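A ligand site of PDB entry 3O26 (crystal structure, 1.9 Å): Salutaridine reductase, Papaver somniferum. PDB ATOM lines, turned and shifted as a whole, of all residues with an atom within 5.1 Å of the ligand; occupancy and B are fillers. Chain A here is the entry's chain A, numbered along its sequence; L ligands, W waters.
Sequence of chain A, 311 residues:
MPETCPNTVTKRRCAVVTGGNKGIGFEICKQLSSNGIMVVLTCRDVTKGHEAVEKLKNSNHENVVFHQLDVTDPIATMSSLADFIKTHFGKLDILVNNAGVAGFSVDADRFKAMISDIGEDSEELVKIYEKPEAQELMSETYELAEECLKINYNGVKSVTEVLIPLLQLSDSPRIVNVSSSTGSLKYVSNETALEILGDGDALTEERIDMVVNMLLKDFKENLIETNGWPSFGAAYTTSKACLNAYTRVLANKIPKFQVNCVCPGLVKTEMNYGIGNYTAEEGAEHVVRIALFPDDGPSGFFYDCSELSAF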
ATOM      1  N   GLY A  19     -27.941  -0.564  28.706  1.00  0.00           N
ATOM      2  CA  GLY A  19     -27.227  -1.809  28.457  1.00  0.00           C
ATOM      3  C   GLY A  19     -27.448  -2.818  29.561  1.00  0.00           C
ATOM      4  O   GLY A  19     -26.491  -3.402  30.094  1.00  0.00           O
ATOM      5  N   GLY A  20     -28.706  -3.060  29.916  1.00  0.00           N
ATOM      6  CA  GLY A  20     -29.019  -3.841  31.102  1.00  0.00           C
ATOM      7  C   GLY A  20     -29.225  -5.334  30.904  1.00  0.00           C
ATOM      8  O   GLY A  20     -29.467  -6.051  31.873  1.00  0.00           O
ATOM      9  N   ASN A  21     -29.130  -5.818  29.662  1.00  0.00           N
ATOM     10  CA  ASN A  21     -29.496  -7.213  29.382  1.00  0.00           C
ATOM     11  C   ASN A  21     -28.439  -8.254  29.721  1.00  0.00           C
ATOM     12  O   ASN A  21     -28.756  -9.426  29.903  1.00  0.00           O
ATOM     13  CB  ASN A  21     -30.014  -7.380  27.946  1.00  0.00           C
ATOM     14  CG  ASN A  21     -29.004  -6.973  26.897  1.00  0.00           C
ATOM     15  OD1 ASN A  21     -28.832  -5.781  26.612  1.00  0.00           O
ATOM     16  ND2 ASN A  21     -28.324  -7.946  26.305  1.00  0.00           N
ATOM     17  N   LYS A  22     -27.178  -7.827  29.826  1.00  0.00           N
ATOM     18  CA  LYS A  22     -26.089  -8.752  30.136  1.00  0.00           C
ATOM     19  C   LYS A  22     -24.922  -8.023  30.778  1.00  0.00           C
ATOM     20  O   LYS A  22     -24.963  -6.808  30.959  1.00  0.00           O
ATOM     21  CB  LYS A  22     -25.623  -9.464  28.863  1.00  0.00           C
ATOM     22  CG  LYS A  22     -24.787  -8.599  27.920  1.00  0.00           C
ATOM     23  CD  LYS A  22     -24.508  -9.327  26.615  1.00  0.00           C
ATOM     24  CE  LYS A  22     -23.468  -8.595  25.772  1.00  0.00           C
ATOM     25  NZ  LYS A  22     -23.208  -9.307  24.494  1.00  0.00           N
ATOM     26  N   GLY A  23     -23.869  -8.772  31.130  1.00  0.00           N
ATOM     27  CA  GLY A  23     -22.637  -8.172  31.616  1.00  0.00           C
ATOM     28  C   GLY A  23     -22.796  -7.395  32.909  1.00  0.00           C
ATOM     29  O   GLY A  23     -23.608  -7.740  33.779  1.00  0.00           O
ATOM     30  N   ILE A  24     -22.018  -6.321  33.040  1.00  0.00           N
ATOM     31  CA  ILE A  24     -22.068  -5.486  34.227  1.00  0.00           C
ATOM     32  C   ILE A  24     -23.451  -4.895  34.420  1.00  0.00           C
ATOM     33  O   ILE A  24     -23.984  -4.888  35.522  1.00  0.00           O
ATOM     34  CB  ILE A  24     -21.038  -4.353  34.170  1.00  0.00           C
ATOM     35  CG1 ILE A  24     -19.631  -4.951  34.013  1.00  0.00           C
ATOM     36  CG2 ILE A  24     -21.137  -3.475  35.409  1.00  0.00           C
ATOM     37  CD1 ILE A  24     -18.555  -3.918  33.726  1.00  0.00           C
ATOM     38  N   GLY A  25     -24.056  -4.423  33.323  1.00  0.00           N
ATOM     39  CA  GLY A  25     -25.365  -3.808  33.359  1.00  0.00           C
ATOM     40  C   GLY A  25     -26.447  -4.685  33.981  1.00  0.00           C
ATOM     41  O   GLY A  25     -27.243  -4.207  34.801  1.00  0.00           O
ATOM     42  N   CYS A  43     -32.495  -1.732  27.252  1.00  0.00           N
ATOM     43  CA  CYS A  43     -31.513  -2.261  26.327  1.00  0.00           C
ATOM     44  C   CYS A  43     -32.090  -2.144  24.923  1.00  0.00           C
ATOM     45  O   CYS A  43     -33.275  -1.852  24.756  1.00  0.00           O
ATOM     46  CB  CYS A  43     -31.144  -3.708  26.669  1.00  0.00           C
ATOM     47  SG  CYS A  43     -32.459  -4.919  26.392  1.00  0.00           S
ATOM     48  N   ARG A  44     -31.258  -2.351  23.908  1.00  0.00           N
ATOM     49  CA  ARG A  44     -31.675  -2.099  22.536  1.00  0.00           C
ATOM     50  C   ARG A  44     -32.486  -3.242  21.913  1.00  0.00           C
ATOM     51  O   ARG A  44     -33.344  -2.992  21.068  1.00  0.00           O
ATOM     52  CB  ARG A  44     -30.471  -1.787  21.648  1.00  0.00           C
ATOM     53  CG  ARG A  44     -29.482  -2.923  21.527  1.00  0.00           C
ATOM     54  CD  ARG A  44     -28.323  -2.517  20.645  1.00  0.00           C
ATOM     55  NE  ARG A  44     -27.198  -3.454  20.758  1.00  0.00           N
ATOM     56  CZ  ARG A  44     -26.048  -3.306  20.117  1.00  0.00           C
ATOM     57  NH1 ARG A  44     -25.858  -2.265  19.306  1.00  0.00           N
ATOM     58  NH2 ARG A  44     -25.084  -4.207  20.278  1.00  0.00           N
ATOM     59  N   ASP A  45     -32.214  -4.471  22.315  1.00  0.00           N
ATOM     60  CA  ASP A  45     -32.900  -5.626  21.740  1.00  0.00           C
ATOM     61  C   ASP A  45     -34.090  -6.016  22.616  1.00  0.00           C
ATOM     62  O   ASP A  45     -33.919  -6.381  23.775  1.00  0.00           O
ATOM     63  CB  ASP A  45     -31.926  -6.793  21.572  1.00  0.00           C
ATOM     64  CG  ASP A  45     -32.550  -7.977  20.835  1.00  0.00           C
ATOM     65  OD1 ASP A  45     -33.476  -8.607  21.389  1.00  0.00           O
ATOM     66  OD2 ASP A  45     -32.106  -8.269  19.710  1.00  0.00           O
ATOM     67  N   LYS A  48     -34.107  -9.618  24.063  1.00  0.00           N
ATOM     68  CA  LYS A  48     -33.092  -9.756  25.102  1.00  0.00           C
ATOM     69  C   LYS A  48     -33.535  -9.051  26.370  1.00  0.00           C
ATOM     70  O   LYS A  48     -33.283  -9.535  27.479  1.00  0.00           O
ATOM     71  CB  LYS A  48     -31.744  -9.246  24.594  1.00  0.00           C
ATOM     72  CG  LYS A  48     -31.077 -10.195  23.590  1.00  0.00           C
ATOM     73  CD  LYS A  48     -29.819  -9.595  22.964  1.00  0.00           C
ATOM     74  CE  LYS A  48     -29.274 -10.510  21.883  1.00  0.00           C
ATOM     75  NZ  LYS A  48     -28.128  -9.896  21.151  1.00  0.00           N
ATOM     76  N   LEU A  69     -34.285   0.901  24.672  1.00  0.00           N
ATOM     77  CA  LEU A  69     -33.407   2.054  24.541  1.00  0.00           C
ATOM     78  C   LEU A  69     -32.112   1.679  23.827  1.00  0.00           C
ATOM     79  O   LEU A  69     -31.302   0.912  24.349  1.00  0.00           O
ATOM     80  CB  LEU A  69     -33.086   2.678  25.913  1.00  0.00           C
ATOM     81  CG  LEU A  69     -32.087   3.848  25.882  1.00  0.00           C
ATOM     82  CD1 LEU A  69     -32.643   4.990  25.054  1.00  0.00           C
ATOM     83  CD2 LEU A  69     -31.723   4.336  27.288  1.00  0.00           C
ATOM     84  N   ASP A  70     -31.953   2.206  22.615  1.00  0.00           N
ATOM     85  CA  ASP A  70     -30.703   2.148  21.895  1.00  0.00           C
ATOM     86  C   ASP A  70     -30.141   3.543  22.044  1.00  0.00           C
ATOM     87  O   ASP A  70     -30.766   4.518  21.623  1.00  0.00           O
ATOM     88  CB  ASP A  70     -30.916   1.804  20.417  1.00  0.00           C
ATOM     89  CG  ASP A  70     -29.616   1.714  19.634  1.00  0.00           C
ATOM     90  OD1 ASP A  70     -28.670   2.487  19.901  1.00  0.00           O
ATOM     91  OD2 ASP A  70     -29.534   0.859  18.730  1.00  0.00           O
ATOM     92  N   VAL A  71     -28.962   3.658  22.660  1.00  0.00           N
ATOM     93  CA  VAL A  71     -28.471   4.989  23.026  1.00  0.00           C
ATOM     94  C   VAL A  71     -28.068   5.804  21.790  1.00  0.00           C
ATOM     95  O   VAL A  71     -27.790   7.006  21.898  1.00  0.00           O
ATOM     96  CB  VAL A  71     -27.301   4.895  24.040  1.00  0.00           C
ATOM     97  CG1 VAL A  71     -27.734   4.096  25.260  1.00  0.00           C
ATOM     98  CG2 VAL A  71     -26.092   4.244  23.375  1.00  0.00           C
ATOM     99  N   THR A  72     -28.033   5.169  20.630  1.00  0.00           N
ATOM    100  CA  THR A  72     -27.692   5.894  19.406  1.00  0.00           C
ATOM    101  C   THR A  72     -28.924   6.450  18.688  1.00  0.00           C
ATOM    102  O   THR A  72     -28.776   7.153  17.687  1.00  0.00           O
ATOM    103  CB  THR A  72     -26.884   5.037  18.407  1.00  0.00           C
ATOM    104  OG1 THR A  72     -27.712   3.971  17.897  1.00  0.00           O
ATOM    105  CG2 THR A  72     -25.639   4.463  19.076  1.00  0.00           C
ATOM    106  N   ASN A  98     -24.291   2.737  31.455  1.00  0.00           N
ATOM    107  CA  ASN A  98     -23.482   1.523  31.403  1.00  0.00           C
ATOM    108  C   ASN A  98     -23.190   1.020  29.988  1.00  0.00           C
ATOM    109  O   ASN A  98     -22.107   0.487  29.711  1.00  0.00           O
ATOM    110  CB  ASN A  98     -24.169   0.419  32.203  1.00  0.00           C
ATOM    111  CG  ASN A  98     -23.569  -0.954  31.944  1.00  0.00           C
ATOM    112  OD1 ASN A  98     -22.528  -1.294  32.497  1.00  0.00           O
ATOM    113  ND2 ASN A  98     -24.223  -1.736  31.085  1.00  0.00           N
ATOM    114  N   ALA A  99     -24.147   1.185  29.086  1.00  0.00           N
ATOM    115  CA  ALA A  99     -23.972   0.715  27.708  1.00  0.00           C
ATOM    116  C   ALA A  99     -22.668   1.189  27.097  1.00  0.00           C
ATOM    117  O   ALA A  99     -22.306   2.364  27.171  1.00  0.00           O
ATOM    118  CB  ALA A  99     -25.153   1.169  26.832  1.00  0.00           C
ATOM    119  N   GLY A 100     -21.952   0.263  26.453  1.00  0.00           N
ATOM    120  CA  GLY A 100     -20.706   0.588  25.781  1.00  0.00           C
ATOM    121  C   GLY A 100     -20.135  -0.570  25.012  1.00  0.00           C
ATOM    122  O   GLY A 100     -20.524  -1.733  25.230  1.00  0.00           O
ATOM    123  N   VAL A 101     -19.214  -0.270  24.103  1.00  0.00           N
ATOM    124  CA  VAL A 101     -18.593  -1.267  23.240  1.00  0.00           C
ATOM    125  C   VAL A 101     -17.092  -1.003  23.124  1.00  0.00           C
ATOM    126  O   VAL A 101     -16.612   0.115  23.396  1.00  0.00           O
ATOM    127  CB  VAL A 101     -19.209  -1.267  21.811  1.00  0.00           C
ATOM    128  CG1 VAL A 101     -20.687  -1.648  21.855  1.00  0.00           C
ATOM    129  CG2 VAL A 101     -18.999   0.088  21.122  1.00  0.00           C
ATOM    130  N   ILE A 151     -21.770   5.356  20.714  1.00  0.00           N
ATOM    131  CA  ILE A 151     -22.383   4.663  21.838  1.00  0.00           C
ATOM    132  C   ILE A 151     -21.777   5.117  23.162  1.00  0.00           C
ATOM    133  O   ILE A 151     -22.509   5.512  24.075  1.00  0.00           O
ATOM    134  CB  ILE A 151     -22.185   3.127  21.717  1.00  0.00           C
ATOM    135  CG1 ILE A 151     -22.935   2.588  20.490  1.00  0.00           C
ATOM    136  CG2 ILE A 151     -22.650   2.443  23.007  1.00  0.00           C
ATOM    137  CD1 ILE A 151     -22.609   1.135  20.166  1.00  0.00           C
ATOM    138  N   ASN A 152     -20.454   5.069  23.249  1.00  0.00           N
ATOM    139  CA  ASN A 152     -19.730   5.340  24.488  1.00  0.00           C
ATOM    140  C   ASN A 152     -19.713   6.813  24.889  1.00  0.00           C
ATOM    141  O   ASN A 152     -19.572   7.120  26.073  1.00  0.00           O
ATOM    142  CB  ASN A 152     -18.277   4.869  24.368  1.00  0.00           C
ATOM    143  CG  ASN A 152     -18.157   3.352  24.302  1.00  0.00           C
ATOM    144  OD1 ASN A 152     -19.150   2.641  24.110  1.00  0.00           O
ATOM    145  ND2 ASN A 152     -16.943   2.861  24.467  1.00  0.00           N
ATOM    146  N   VAL A 178     -20.144   4.603  33.610  1.00  0.00           N
ATOM    147  CA  VAL A 178     -19.197   3.518  33.738  1.00  0.00           C
ATOM    148  C   VAL A 178     -18.050   3.752  32.784  1.00  0.00           C
ATOM    149  O   VAL A 178     -18.216   3.694  31.555  1.00  0.00           O
ATOM    150  CB  VAL A 178     -19.862   2.150  33.476  1.00  0.00           C
ATOM    151  CG1 VAL A 178     -18.865   1.029  33.767  1.00  0.00           C
ATOM    152  CG2 VAL A 178     -21.129   2.011  34.306  1.00  0.00           C
ATOM    153  N   SER A 179     -16.871   4.029  33.345  1.00  0.00           N
ATOM    154  CA  SER A 179     -15.724   4.403  32.530  1.00  0.00           C
ATOM    155  C   SER A 179     -14.644   3.318  32.616  1.00  0.00           C
ATOM    156  O   SER A 179     -14.902   2.221  33.122  1.00  0.00           O
ATOM    157  CB  SER A 179     -15.154   5.744  32.996  1.00  0.00           C
ATOM    158  OG  SER A 179     -14.222   6.279  32.070  1.00  0.00           O
ATOM    159  N   SER A 180     -13.449   3.633  32.127  1.00  0.00           N
ATOM    160  CA  SER A 180     -12.332   2.695  32.187  1.00  0.00           C
ATOM    161  C   SER A 180     -11.043   3.447  32.508  1.00  0.00           C
ATOM    162  O   SER A 180     -10.870   4.600  32.108  1.00  0.00           O
ATOM    163  CB  SER A 180     -12.190   1.957  30.851  1.00  0.00           C
ATOM    164  OG  SER A 180     -10.874   1.456  30.668  1.00  0.00           O
ATOM    165  N   TYR A 236     -11.843   3.513  21.731  1.00  0.00           N
ATOM    166  CA  TYR A 236     -12.296   3.204  23.093  1.00  0.00           C
ATOM    167  C   TYR A 236     -11.660   4.133  24.118  1.00  0.00           C
ATOM    168  O   TYR A 236     -12.358   4.746  24.926  1.00  0.00           O
ATOM    169  CB  TYR A 236     -11.955   1.753  23.469  1.00  0.00           C
ATOM    170  CG  TYR A 236     -12.537   1.304  24.806  1.00  0.00           C
ATOM    171  CD1 TYR A 236     -13.847   0.856  24.884  1.00  0.00           C
ATOM    172  CD2 TYR A 236     -11.778   1.309  25.969  1.00  0.00           C
ATOM    173  CE1 TYR A 236     -14.403   0.434  26.084  1.00  0.00           C
ATOM    174  CE2 TYR A 236     -12.313   0.868  27.183  1.00  0.00           C
ATOM    175  CZ  TYR A 236     -13.621   0.452  27.233  1.00  0.00           C
ATOM    176  OH  TYR A 236     -14.170   0.020  28.413  1.00  0.00           O
ATOM    177  N   LYS A 240     -13.591   7.070  26.402  1.00  0.00           N
ATOM    178  CA  LYS A 240     -13.689   7.085  27.868  1.00  0.00           C
ATOM    179  C   LYS A 240     -13.014   8.318  28.486  1.00  0.00           C
ATOM    180  O   LYS A 240     -13.437   8.817  29.523  1.00  0.00           O
ATOM    181  CB  LYS A 240     -13.132   5.784  28.474  1.00  0.00           C
ATOM    182  CG  LYS A 240     -13.920   4.520  28.096  1.00  0.00           C
ATOM    183  CD  LYS A 240     -15.379   4.571  28.554  1.00  0.00           C
ATOM    184  CE  LYS A 240     -16.022   3.194  28.388  1.00  0.00           C
ATOM    185  NZ  LYS A 240     -17.411   3.144  28.877  1.00  0.00           N
ATOM    186  N   PRO A 264     -14.786   0.052  36.799  1.00  0.00           N
ATOM    187  CA  PRO A 264     -15.117  -1.180  37.529  1.00  0.00           C
ATOM    188  C   PRO A 264     -13.982  -2.206  37.609  1.00  0.00           C
ATOM    189  O   PRO A 264     -14.195  -3.257  38.210  1.00  0.00           O
ATOM    190  CB  PRO A 264     -16.281  -1.755  36.731  1.00  0.00           C
ATOM    191  CG  PRO A 264     -16.029  -1.273  35.323  1.00  0.00           C
ATOM    192  CD  PRO A 264     -15.481   0.120  35.489  1.00  0.00           C
ATOM    193  N   GLY A 265     -12.818  -1.905  37.041  1.00  0.00           N
ATOM    194  CA  GLY A 265     -11.761  -2.899  36.941  1.00  0.00           C
ATOM    195  C   GLY A 265     -11.998  -3.817  35.748  1.00  0.00           C
ATOM    196  O   GLY A 265     -12.997  -3.651  35.032  1.00  0.00           O
ATOM    197  N   LEU A 266     -11.111  -4.785  35.520  1.00  0.00           N
ATOM    198  CA  LEU A 266     -11.303  -5.687  34.389  1.00  0.00           C
ATOM    199  C   LEU A 266     -12.283  -6.797  34.755  1.00  0.00           C
ATOM    200  O   LEU A 266     -12.022  -7.590  35.658  1.00  0.00           O
ATOM    201  CB  LEU A 266      -9.964  -6.260  33.880  1.00  0.00           C
ATOM    202  CG  LEU A 266     -10.040  -6.919  32.499  1.00  0.00           C
ATOM    203  CD1 LEU A 266     -10.217  -5.878  31.391  1.00  0.00           C
ATOM    204  CD2 LEU A 266      -8.806  -7.774  32.220  1.00  0.00           C
ATOM    205  N   VAL A 267     -13.412  -6.833  34.052  1.00  0.00           N
ATOM    206  CA  VAL A 267     -14.532  -7.691  34.420  1.00  0.00           C
ATOM    207  C   VAL A 267     -14.792  -8.776  33.388  1.00  0.00           C
ATOM    208  O   VAL A 267     -14.748  -8.530  32.179  1.00  0.00           O
ATOM    209  CB  VAL A 267     -15.820  -6.852  34.584  1.00  0.00           C
ATOM    210  CG1 VAL A 267     -16.951  -7.714  35.092  1.00  0.00           C
ATOM    211  CG2 VAL A 267     -15.574  -5.667  35.525  1.00  0.00           C
ATOM    212  N   THR A 269     -16.778 -10.313  31.266  1.00  0.00           N
ATOM    213  CA  THR A 269     -18.014 -10.232  30.503  1.00  0.00           C
ATOM    214  C   THR A 269     -17.679 -10.577  29.075  1.00  0.00           C
ATOM    215  O   THR A 269     -16.505 -10.773  28.731  1.00  0.00           O
ATOM    216  CB  THR A 269     -18.588  -8.801  30.525  1.00  0.00           C
ATOM    217  OG1 THR A 269     -17.705  -7.942  29.788  1.00  0.00           O
ATOM    218  CG2 THR A 269     -18.732  -8.277  31.954  1.00  0.00           C
ATOM    219  N   GLU A 270     -18.701 -10.615  28.221  1.00  0.00           N
ATOM    220  CA  GLU A 270     -18.505 -10.879  26.806  1.00  0.00           C
ATOM    221  C   GLU A 270     -17.683  -9.797  26.106  1.00  0.00           C
ATOM    222  O   GLU A 270     -17.135 -10.035  25.037  1.00  0.00           O
ATOM    223  CB  GLU A 270     -19.858 -11.079  26.097  1.00  0.00           C
ATOM    224  CG  GLU A 270     -20.577 -12.354  26.513  1.00  0.00           C
ATOM    225  CD  GLU A 270     -21.967 -12.500  25.891  1.00  0.00           C
ATOM    226  OE1 GLU A 270     -22.317 -11.720  24.978  1.00  0.00           O
ATOM    227  OE2 GLU A 270     -22.710 -13.415  26.319  1.00  0.00           O
ATOM    228  N   MET A 271     -17.590  -8.609  26.716  1.00  0.00           N
ATOM    229  CA  MET A 271     -16.728  -7.564  26.136  1.00  0.00           C
ATOM    230  C   MET A 271     -15.311  -8.091  26.025  1.00  0.00           C
ATOM    231  O   MET A 271     -14.596  -7.749  25.082  1.00  0.00           O
ATOM    232  CB  MET A 271     -16.750  -6.254  26.941  1.00  0.00           C
ATOM    233  CG  MET A 271     -15.835  -5.150  26.365  1.00  0.00           C
ATOM    234  SD  MET A 271     -15.899  -3.503  27.146  1.00  0.00           S
ATOM    235  CE  MET A 271     -17.453  -2.905  26.543  1.00  0.00           C
ATOM    236  N   ASN A 272     -14.901  -8.923  26.979  1.00  0.00           N
ATOM    237  CA  ASN A 272     -13.538  -9.450  27.011  1.00  0.00           C
ATOM    238  C   ASN A 272     -13.489 -10.935  26.695  1.00  0.00           C
ATOM    239  O   ASN A 272     -12.500 -11.602  27.006  1.00  0.00           O
ATOM    240  CB  ASN A 272     -12.909  -9.245  28.390  1.00  0.00           C
ATOM    241  CG  ASN A 272     -12.792  -7.788  28.772  1.00  0.00           C
ATOM    242  OD1 ASN A 272     -12.394  -6.959  27.956  1.00  0.00           O
ATOM    243  ND2 ASN A 272     -13.092  -7.476  30.022  1.00  0.00           N
HETATM  244  P1  LIG L   1     -21.031  -6.281  27.652  1.00  0.00           P
HETATM  245  O1  LIG L   1     -21.155  -7.572  28.333  1.00  0.00           O
HETATM  246  O2  LIG L   1     -20.496  -6.473  26.111  1.00  0.00           O
HETATM  247  O3  LIG L   1     -22.463  -5.502  27.668  1.00  0.00           O
HETATM  248  C1  LIG L   1     -22.580  -4.335  26.898  1.00  0.00           C
HETATM  249  C2  LIG L   1     -24.014  -3.843  27.105  1.00  0.00           C
HETATM  250  O4  LIG L   1     -24.137  -2.577  26.389  1.00  0.00           O
HETATM  251  C3  LIG L   1     -24.976  -4.835  26.456  1.00  0.00           C
HETATM  252  O5  LIG L   1     -26.206  -4.784  27.139  1.00  0.00           O
HETATM  253  C4  LIG L   1     -25.124  -4.281  25.075  1.00  0.00           C
HETATM  254  O6  LIG L   1     -26.333  -4.664  24.491  1.00  0.00           O
HETATM  255  C5  LIG L   1     -25.215  -2.814  25.452  1.00  0.00           C
HETATM  256  N1  LIG L   1     -25.055  -1.985  24.275  1.00  0.00           N
HETATM  257  C6  LIG L   1     -24.021  -2.029  23.221  1.00  0.00           C
HETATM  258  N2  LIG L   1     -24.380  -0.996  22.236  1.00  0.00           N
HETATM  259  C7  LIG L   1     -25.630  -0.369  22.686  1.00  0.00           C
HETATM  260  C8  LIG L   1     -26.515   0.661  22.097  1.00  0.00           C
HETATM  261  N3  LIG L   1     -26.206   1.211  20.807  1.00  0.00           N
HETATM  262  N4  LIG L   1     -27.694   1.073  22.829  1.00  0.00           N
HETATM  263  C9  LIG L   1     -28.053   0.496  24.127  1.00  0.00           C
HETATM  264  N5  LIG L   1     -27.220  -0.602  24.670  1.00  0.00           N
HETATM  265  C10 LIG L   1     -26.036  -0.993  23.951  1.00  0.00           C
HETATM  266  O7  LIG L   1     -19.904  -5.273  28.247  1.00  0.00           O
HETATM  267  P2  LIG L   1     -19.699  -4.861  29.808  1.00  0.00           P
HETATM  268  O8  LIG L   1     -20.825  -5.272  30.647  1.00  0.00           O
HETATM  269  O9  LIG L   1     -18.235  -5.479  30.186  1.00  0.00           O
HETATM  270  O10 LIG L   1     -19.551  -3.200  29.745  1.00  0.00           O
HETATM  271  C11 LIG L   1     -20.517  -2.340  30.299  1.00  0.00           C
HETATM  272  C12 LIG L   1     -19.796  -0.994  30.553  1.00  0.00           C
HETATM  273  O11 LIG L   1     -18.634  -1.258  31.393  1.00  0.00           O
HETATM  274  C13 LIG L   1     -19.231  -0.457  29.237  1.00  0.00           C
HETATM  275  O12 LIG L   1     -19.376   0.928  29.178  1.00  0.00           O
HETATM  276  C14 LIG L   1     -17.767  -0.797  29.300  1.00  0.00           C
HETATM  277  O13 LIG L   1     -16.961   0.071  28.535  1.00  0.00           O
HETATM  278  C15 LIG L   1     -17.522  -0.549  30.791  1.00  0.00           C
HETATM  279  N6  LIG L   1     -16.297  -1.183  31.228  1.00  0.00           N
HETATM  280  C16 LIG L   1     -16.124  -2.642  31.075  1.00  0.00           C
HETATM  281  C17 LIG L   1     -14.844  -3.309  31.563  1.00  0.00           C
HETATM  282  C18 LIG L   1     -14.674  -4.808  31.407  1.00  0.00           C
HETATM  283  O14 LIG L   1     -13.630  -5.294  31.677  1.00  0.00           O
HETATM  284  N7  LIG L   1     -15.816  -5.618  31.023  1.00  0.00           N
HETATM  285  C19 LIG L   1     -13.769  -2.502  32.198  1.00  0.00           C
HETATM  286  C20 LIG L   1     -13.957  -1.026  32.359  1.00  0.00           C
HETATM  287  C21 LIG L   1     -15.236  -0.368  31.870  1.00  0.00           C
HETATM  288  P3  LIG L   1     -26.327  -5.942  23.459  1.00  0.00           P
HETATM  289  O15 LIG L   1     -25.105  -5.942  22.643  1.00  0.00           O
HETATM  290  O16 LIG L   1     -26.437  -7.316  24.354  1.00  0.00           O
HETATM  291  O17 LIG L   1     -27.620  -5.705  22.486  1.00  0.00           O
HETATM  292  O   HOH W   1     -25.875  -9.644  23.323  1.00  0.00           O
HETATM  293  O   HOH W   2     -23.407  -4.407  30.474  1.00  0.00           O
HETATM  294  O   HOH W   3     -21.089   3.959  29.269  1.00  0.00           O
HETATM  295  O   HOH W   4     -20.648  -7.837  23.788  1.00  0.00           O
HETATM  296  O   HOH W   5     -21.535 -10.193  28.843  1.00  0.00           O
HETATM  297  O   HOH W   6     -12.363  -1.857  29.218  1.00  0.00           O
HETATM  298  O   HOH W   7     -22.247  -4.955  22.749  1.00  0.00           O
HETATM  299  O   HOH W   8     -19.941  -4.436  24.433  1.00  0.00           O
HETATM  300  O   HOH W   9     -28.537  -2.904  24.998  1.00  0.00           O
HETATM  301  O   HOH W  10     -29.967  -5.606  23.806  1.00  0.00           O
HETATM  302  O   HOH W  11     -23.884  -7.911  20.996  1.00  0.00           O
HETATM  303  O   HOH W  12     -28.387  -7.081  20.272  1.00  0.00           O
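Water W1 lies within hydrogen-bond range of O16 of the ligand (2.6 Å), NZ of Lys 22 (2.9 Å) and NZ of Lys 48 (3.1 Å).
Water W9 lies within hydrogen-bond range of N5 of the ligand, N of Arg 44 and OD1 of Asn 21.
Water W10 lies within hydrogen-bond range of an oxygen (O17) of the ligand (2.7 Å), the backbone NH of Asp 45 (2.9 Å), the side-chain amide oxygen of Asn 21 (3.0 Å) and the side-chain sulfur of Cys 43 (3.7 Å).
Water W5 lies within hydrogen-bond range of O1 of the ligand (2.7 Å) and N of Glu 270 (2.9 Å).
Water W12 lies within hydrogen-bond range of O17 of the ligand (2.7 Å) and NZ of Lys 48 (3.0 Å).
Water W3 lies within hydrogen-bond range of the backbone carbonyl oxygen of Ala 99 and an oxygen (O12) of the ligand.
Gly 23 touches the ligand (CA to O8, 3.6 Å).
O of Leu 69 touches C9 of the ligand (3.3 Å).
Thr 72 touches the ligand (CG2 to N3, 3.7 Å).
CB of Ala 99 touches N5 of the ligand (3.5 Å).
N of Gly 100 touches O4 of the ligand (3.6 Å).
Val 101 touches the ligand (CG1 to C6, 3.6 Å).
Ile 151 touches the ligand (CD1 to N2, 3.5 Å).
Val 178 touches the ligand (CG1 to O11, 3.3 Å).
Ser 179 touches the ligand.
Ser 180 touches the ligand (CB to C20, 3.8 Å).
Pro 264 touches the ligand (CG to C20, 3.6 Å).
O of Gly 265 touches C19 of the ligand, 3.2 Å away.
CD1 of Leu 266 touches O14 of the ligand, 3.5 Å away.
Glu 270 touches the ligand (N to O1, 3.9 Å).
CE of Met 271 touches C14 of the ligand, at 3.5 Å.
Within 4 Å of the ligand: Gly 19, Asn 21, Lys 22, Gly 23, Ile 24, Arg 44, Leu 69, Asp 70, Val 71, Thr 72, Asn 98, Ala 99, Gly 100, Val 101, Ile 151, Val 178, Ser 179, Ser 180, Tyr 236, Lys 240, Pro 264, Gly 265, Leu 266, Val 267, Thr 269, Glu 270, Met 271 and Asn 272.
The side-chain hydroxyl of Thr 269 lies within hydrogen-bond range of an oxygen (O9) of the ligand (2.6 Å).
ND2 of Asn 21 is in hydrogen-bond range of O16 of the ligand (2.8 Å).
The side-chain amide nitrogen (ND2) of Asn 272 lies within hydrogen-bond range of an oxygen (O14) of the ligand (2.8 Å).
The side-chain hydroxyl (OH) of Tyr 236 lies within hydrogen-bond range of an oxygen (O13) of the ligand (2.8 Å).
An oxygen (O12) of the ligand is in hydrogen-bond range of the backbone carbonyl oxygen of Asn 98.
The backbone NH (N) of Val 267 is in hydrogen-bond range of an oxygen (O14) of the ligand (2.8 Å).
The backbone carbonyl oxygen of Val 267 lies within hydrogen-bond range of a nitrogen (N7) of the ligand (3.3 Å).
NE of Arg 44 is in salt-bridge range of O17 of the ligand.
O8 of the ligand sits at hydrogen-bond distance from N of Ile 24.
N of Val 71 is in hydrogen-bond range of N4 of the ligand.
The side-chain carboxylate (OD1) of Asp 70 sits at hydrogen-bond distance from a nitrogen (N3) of the ligand (2.9 Å).
NZ of Lys 240 lies within hydrogen-bond range of O12 of the ligand (3.0 Å).
O5 of the ligand is in hydrogen-bond range of O of Gly 19, 3.3 Å away.
O16 of the ligand lies within salt-bridge range of NZ of Lys 22 (3.8 Å).
N of Met 271 sits close to OG1 of Thr 269 (3.1 Å).
The side-chain amide oxygen of Asn 21 lies close to the side-chain sulfur of Cys 43 (3.7 Å).
O of Val 267 sits at hydrogen-bond distance from ND2 of Asn 272 (2.9 Å).
The backbone carbonyl oxygen (O) of Gly 19 is in hydrogen-bond range of the side-chain amide nitrogen (ND2) of Asn 98 (3.0 Å).
The backbone NH (N) of Arg 44 is in hydrogen-bond range of the backbone carbonyl oxygen (O) of Leu 69 (3.3 Å).
The backbone NH (N) of Leu 69 is in hydrogen-bond range of the backbone carbonyl oxygen (O) of Cys 43.
The side-chain carboxylate (OE1) of Glu 270 is in salt-bridge range of the side-chain amino group (NZ) of Lys 22.
The side-chain amide oxygen of Asn 152 lies within hydrogen-bond range of the backbone NH of Val 101, 2.9 Å away.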
